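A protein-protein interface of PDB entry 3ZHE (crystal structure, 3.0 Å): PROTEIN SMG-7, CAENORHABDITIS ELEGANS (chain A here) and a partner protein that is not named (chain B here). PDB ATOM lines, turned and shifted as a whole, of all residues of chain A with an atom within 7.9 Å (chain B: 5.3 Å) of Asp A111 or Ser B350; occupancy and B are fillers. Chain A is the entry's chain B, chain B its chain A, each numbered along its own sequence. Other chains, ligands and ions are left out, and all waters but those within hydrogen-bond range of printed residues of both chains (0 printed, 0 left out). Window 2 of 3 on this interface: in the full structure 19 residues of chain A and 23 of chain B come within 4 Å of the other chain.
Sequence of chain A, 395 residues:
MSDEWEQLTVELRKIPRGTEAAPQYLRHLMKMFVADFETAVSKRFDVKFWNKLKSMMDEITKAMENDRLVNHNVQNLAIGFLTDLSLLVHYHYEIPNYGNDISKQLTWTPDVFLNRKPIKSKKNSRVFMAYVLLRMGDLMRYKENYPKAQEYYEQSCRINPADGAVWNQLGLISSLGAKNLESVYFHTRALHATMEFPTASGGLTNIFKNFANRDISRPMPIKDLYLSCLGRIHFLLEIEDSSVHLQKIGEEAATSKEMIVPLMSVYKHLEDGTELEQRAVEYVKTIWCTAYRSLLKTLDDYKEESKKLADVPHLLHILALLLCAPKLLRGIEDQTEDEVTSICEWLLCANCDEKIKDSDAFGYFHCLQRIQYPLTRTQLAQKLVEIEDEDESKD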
ATOM      1  N   TRP A 108      18.066  -5.157 -31.746  1.00  0.00           N
ATOM      2  CA  TRP A 108      17.355  -6.222 -31.038  1.00  0.00           C
ATOM      3  C   TRP A 108      15.863  -6.131 -31.334  1.00  0.00           C
ATOM      4  O   TRP A 108      15.465  -5.666 -32.401  1.00  0.00           O
ATOM      5  CB  TRP A 108      17.624  -6.189 -29.530  1.00  0.00           C
ATOM      6  CG  TRP A 108      18.971  -6.721 -29.155  1.00  0.00           C
ATOM      7  CD1 TRP A 108      19.790  -7.497 -29.925  1.00  0.00           C
ATOM      8  CD2 TRP A 108      19.663  -6.510 -27.918  1.00  0.00           C
ATOM      9  NE1 TRP A 108      20.948  -7.785 -29.239  1.00  0.00           N
ATOM     10  CE2 TRP A 108      20.894  -7.190 -28.006  1.00  0.00           C
ATOM     11  CE3 TRP A 108      19.359  -5.814 -26.744  1.00  0.00           C
ATOM     12  CZ2 TRP A 108      21.822  -7.194 -26.964  1.00  0.00           C
ATOM     13  CZ3 TRP A 108      20.281  -5.817 -25.710  1.00  0.00           C
ATOM     14  CH2 TRP A 108      21.498  -6.503 -25.826  1.00  0.00           C
ATOM     15  N   THR A 109      15.042  -6.583 -30.394  1.00  0.00           N
ATOM     16  CA  THR A 109      13.595  -6.562 -30.565  1.00  0.00           C
ATOM     17  C   THR A 109      12.935  -6.006 -29.309  1.00  0.00           C
ATOM     18  O   THR A 109      13.529  -6.038 -28.233  1.00  0.00           O
ATOM     19  CB  THR A 109      13.049  -7.971 -30.862  1.00  0.00           C
ATOM     20  OG1 THR A 109      13.497  -8.883 -29.852  1.00  0.00           O
ATOM     21  CG2 THR A 109      13.534  -8.451 -32.223  1.00  0.00           C
ATOM     22  N   PRO A 110      11.707  -5.478 -29.438  1.00  0.00           N
ATOM     23  CA  PRO A 110      11.006  -4.952 -28.262  1.00  0.00           C
ATOM     24  C   PRO A 110      10.694  -6.027 -27.221  1.00  0.00           C
ATOM     25  O   PRO A 110      10.340  -5.696 -26.091  1.00  0.00           O
ATOM     26  CB  PRO A 110       9.703  -4.404 -28.850  1.00  0.00           C
ATOM     27  CG  PRO A 110       9.995  -4.159 -30.282  1.00  0.00           C
ATOM     28  CD  PRO A 110      10.970  -5.214 -30.686  1.00  0.00           C
ATOM     29  N   ASP A 111      10.830  -7.294 -27.598  1.00  0.00           N
ATOM     30  CA  ASP A 111      10.471  -8.396 -26.710  1.00  0.00           C
ATOM     31  C   ASP A 111      11.499  -8.655 -25.609  1.00  0.00           C
ATOM     32  O   ASP A 111      11.227  -9.406 -24.676  1.00  0.00           O
ATOM     33  CB  ASP A 111      10.247  -9.681 -27.513  1.00  0.00           C
ATOM     34  CG  ASP A 111       9.118  -9.553 -28.519  1.00  0.00           C
ATOM     35  OD1 ASP A 111       9.375  -9.065 -29.641  1.00  0.00           O
ATOM     36  OD2 ASP A 111       7.976  -9.946 -28.196  1.00  0.00           O
ATOM     37  N   VAL A 112      12.672  -8.039 -25.711  1.00  0.00           N
ATOM     38  CA  VAL A 112      13.760  -8.349 -24.787  1.00  0.00           C
ATOM     39  C   VAL A 112      14.000  -7.283 -23.715  1.00  0.00           C
ATOM     40  O   VAL A 112      14.907  -7.419 -22.894  1.00  0.00           O
ATOM     41  CB  VAL A 112      15.081  -8.626 -25.539  1.00  0.00           C
ATOM     42  CG1 VAL A 112      14.896  -9.753 -26.543  1.00  0.00           C
ATOM     43  CG2 VAL A 112      15.580  -7.369 -26.231  1.00  0.00           C
ATOM     44  N   PHE A 113      13.192  -6.227 -23.723  1.00  0.00           N
ATOM     45  CA  PHE A 113      13.352  -5.148 -22.753  1.00  0.00           C
ATOM     46  C   PHE A 113      12.187  -5.113 -21.763  1.00  0.00           C
ATOM     47  O   PHE A 113      11.086  -5.565 -22.072  1.00  0.00           O
ATOM     48  CB  PHE A 113      13.489  -3.801 -23.470  1.00  0.00           C
ATOM     49  CG  PHE A 113      14.489  -3.810 -24.596  1.00  0.00           C
ATOM     50  CD1 PHE A 113      15.830  -4.054 -24.351  1.00  0.00           C
ATOM     51  CD2 PHE A 113      14.087  -3.562 -25.899  1.00  0.00           C
ATOM     52  CE1 PHE A 113      16.748  -4.060 -25.383  1.00  0.00           C
ATOM     53  CE2 PHE A 113      15.003  -3.565 -26.935  1.00  0.00           C
ATOM     54  CZ  PHE A 113      16.334  -3.815 -26.676  1.00  0.00           C
ATOM     55  N   LEU A 114      12.437  -4.580 -20.570  1.00  0.00           N
ATOM     56  CA  LEU A 114      11.419  -4.531 -19.523  1.00  0.00           C
ATOM     57  C   LEU A 114      10.783  -3.151 -19.398  1.00  0.00           C
ATOM     58  O   LEU A 114       9.876  -2.803 -20.154  1.00  0.00           O
ATOM     59  CB  LEU A 114      12.021  -4.938 -18.179  1.00  0.00           C
ATOM     60  N   ARG A 116      11.142   0.510 -19.948  1.00  0.00           N
ATOM     61  CA  ARG A 116      11.848   1.577 -20.644  1.00  0.00           C
ATOM     62  C   ARG A 116      11.132   2.912 -20.478  1.00  0.00           C
ATOM     63  O   ARG A 116       9.905   2.978 -20.535  1.00  0.00           O
ATOM     64  CB  ARG A 116      11.983   1.246 -22.133  1.00  0.00           C
ATOM     65  CG  ARG A 116      12.665  -0.079 -22.417  1.00  0.00           C
ATOM     66  CD  ARG A 116      13.053  -0.197 -23.883  1.00  0.00           C
ATOM     67  NE  ARG A 116      11.923  -0.521 -24.751  1.00  0.00           N
ATOM     68  CZ  ARG A 116      12.016  -0.672 -26.069  1.00  0.00           C
ATOM     69  NH1 ARG A 116      13.185  -0.524 -26.675  1.00  0.00           N
ATOM     70  NH2 ARG A 116      10.940  -0.970 -26.784  1.00  0.00           N
ATOM     71  N   ASP B 138      15.440 -15.230 -28.072  1.00  0.00           N
ATOM     72  CA  ASP B 138      14.487 -14.791 -29.085  1.00  0.00           C
ATOM     73  C   ASP B 138      14.836 -15.400 -30.440  1.00  0.00           C
ATOM     74  O   ASP B 138      13.980 -15.526 -31.318  1.00  0.00           O
ATOM     75  CB  ASP B 138      14.460 -13.264 -29.178  1.00  0.00           C
ATOM     76  CG  ASP B 138      13.367 -12.757 -30.099  1.00  0.00           C
ATOM     77  OD1 ASP B 138      12.305 -13.410 -30.178  1.00  0.00           O
ATOM     78  OD2 ASP B 138      13.569 -11.708 -30.746  1.00  0.00           O
ATOM     79  N   SER B 348       0.685 -13.145 -35.454  1.00  0.00           N
ATOM     80  CA  SER B 348       2.137 -13.184 -35.597  1.00  0.00           C
ATOM     81  C   SER B 348       2.842 -12.417 -34.481  1.00  0.00           C
ATOM     82  O   SER B 348       3.781 -11.662 -34.727  1.00  0.00           O
ATOM     83  CB  SER B 348       2.558 -12.649 -36.969  1.00  0.00           C
ATOM     84  OG  SER B 348       3.873 -13.057 -37.295  1.00  0.00           O
ATOM     85  N   ILE B 349       2.374 -12.612 -33.252  1.00  0.00           N
ATOM     86  CA  ILE B 349       2.966 -11.957 -32.091  1.00  0.00           C
ATOM     87  C   ILE B 349       4.077 -12.827 -31.511  1.00  0.00           C
ATOM     88  O   ILE B 349       3.907 -14.036 -31.355  1.00  0.00           O
ATOM     89  CB  ILE B 349       1.903 -11.677 -31.007  1.00  0.00           C
ATOM     90  CG1 ILE B 349       0.846 -10.709 -31.538  1.00  0.00           C
ATOM     91  CG2 ILE B 349       2.546 -11.111 -29.750  1.00  0.00           C
ATOM     92  CD1 ILE B 349       1.396  -9.344 -31.892  1.00  0.00           C
ATOM     93  N   SER B 350       5.216 -12.213 -31.203  1.00  0.00           N
ATOM     94  CA  SER B 350       6.340 -12.943 -30.630  1.00  0.00           C
ATOM     95  C   SER B 350       6.022 -13.423 -29.217  1.00  0.00           C
ATOM     96  O   SER B 350       5.424 -12.695 -28.423  1.00  0.00           O
ATOM     97  CB  SER B 350       7.604 -12.080 -30.626  1.00  0.00           C
ATOM     98  OG  SER B 350       8.698 -12.781 -30.057  1.00  0.00           O
ATOM     99  N   MET B 351       6.424 -14.654 -28.916  1.00  0.00           N
ATOM    100  CA  MET B 351       6.182 -15.257 -27.609  1.00  0.00           C
ATOM    101  C   MET B 351       7.347 -15.012 -26.659  1.00  0.00           C
ATOM    102  O   MET B 351       7.300 -15.412 -25.498  1.00  0.00           O
ATOM    103  CB  MET B 351       5.962 -16.765 -27.751  1.00  0.00           C
ATOM    104  CG  MET B 351       4.738 -17.147 -28.562  1.00  0.00           C
ATOM    105  SD  MET B 351       3.196 -16.656 -27.768  1.00  0.00           S
ATOM    106  CE  MET B 351       3.342 -17.495 -26.192  1.00  0.00           C
ATOM    107  N   THR B 352       8.386 -14.352 -27.162  1.00  0.00           N
ATOM    108  CA  THR B 352       9.632 -14.173 -26.419  1.00  0.00           C
ATOM    109  C   THR B 352       9.449 -13.483 -25.066  1.00  0.00           C
ATOM    110  O   THR B 352       9.910 -13.983 -24.040  1.00  0.00           O
ATOM    111  CB  THR B 352      10.665 -13.391 -27.255  1.00  0.00           C
ATOM    112  OG1 THR B 352      11.019 -14.155 -28.415  1.00  0.00           O
ATOM    113  CG2 THR B 352      11.918 -13.112 -26.443  1.00  0.00           C
ATOM    114  N   SER B 353       8.774 -12.337 -25.075  1.00  0.00           N
ATOM    115  CA  SER B 353       8.564 -11.541 -23.868  1.00  0.00           C
ATOM    116  C   SER B 353       7.798 -12.316 -22.802  1.00  0.00           C
ATOM    117  O   SER B 353       8.217 -12.391 -21.642  1.00  0.00           O
ATOM    118  CB  SER B 353       7.816 -10.251 -24.215  1.00  0.00           C
ATOM    119  OG  SER B 353       7.549  -9.486 -23.053  1.00  0.00           O
ATOM    120  N   LEU B 356      10.041 -15.175 -21.400  1.00  0.00           N
ATOM    121  CA  LEU B 356      11.100 -14.732 -20.499  1.00  0.00           C
ATOM    122  C   LEU B 356      10.568 -14.221 -19.165  1.00  0.00           C
ATOM    123  O   LEU B 356      11.061 -14.602 -18.102  1.00  0.00           O
ATOM    124  CB  LEU B 356      11.939 -13.637 -21.161  1.00  0.00           C
ATOM    125  CG  LEU B 356      12.767 -14.058 -22.371  1.00  0.00           C
ATOM    126  CD1 LEU B 356      13.531 -12.870 -22.930  1.00  0.00           C
ATOM    127  CD2 LEU B 356      13.717 -15.177 -21.987  1.00  0.00           C
ATOM    128  N   PHE B 367      -2.638 -10.888 -28.661  1.00  0.00           N
ATOM    129  CA  PHE B 367      -1.907 -11.915 -27.929  1.00  0.00           C
ATOM    130  C   PHE B 367      -2.814 -13.084 -27.571  1.00  0.00           C
ATOM    131  O   PHE B 367      -2.475 -14.241 -27.818  1.00  0.00           O
ATOM    132  CB  PHE B 367      -1.284 -11.323 -26.664  1.00  0.00           C
ATOM    133  CG  PHE B 367      -0.548 -12.326 -25.825  1.00  0.00           C
ATOM    134  CD1 PHE B 367       0.728 -12.731 -26.174  1.00  0.00           C
ATOM    135  CD2 PHE B 367      -1.130 -12.861 -24.687  1.00  0.00           C
ATOM    136  CE1 PHE B 367       1.408 -13.654 -25.406  1.00  0.00           C
ATOM    137  CE2 PHE B 367      -0.455 -13.784 -23.915  1.00  0.00           C
ATOM    138  CZ  PHE B 367       0.816 -14.179 -24.273  1.00  0.00           C
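The side-chain hydroxyl (OG) of Ser B350 lies close to the side-chain carboxylate (OD2) of Asp A111 (3.5 Å).
OD2 of Asp B138 sits at hydrogen-bond distance from OG1 of Thr A109 (3.0 Å).
The side-chain hydroxyl of Ser B350 lies within hydrogen-bond range of the side-chain hydroxyl of Thr B352 (3.2 Å).
Asp A111 touches Thr B352 (CB to CB, 3.7 Å).
O of Asp A111 touches CA of Ser B353, 3.5 Å away.
Of the printed residues of chain B, Thr A109 touches Asp B138.
Printed residues of chain B within 4 Å of Asp A111: Ser B350, Thr B352 and Ser B353.
Of chain A, only Asp A111 comes within 4 Å of Ser B350.
Printed residues of chain A within 4 Å of Thr B352: Asp A111.
Printed residues of chain A within 4 Å of Ser B353: Asp A111 (3.5 Å).
Phe B367 touches none of the printed residues of chain A.
The nearest residue of chain B that does not touch Asp A111 is Leu B356 (4.5 Å).
The nearest residue of chain A that does not touch Ser B350 is Thr A109 (6.2 Å).
Printed residues of chain B that touch a printed residue of chain A: Asp B138, Ser B350, Thr B352 and Ser B353.
Of the 8 printed residues of chain A, 2 touch a printed residue of chain B.
Among the printed residues, no Asp or Glu carboxylate lies within 4 Å of a Lys or Arg side-chain nitrogen of the other chain.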
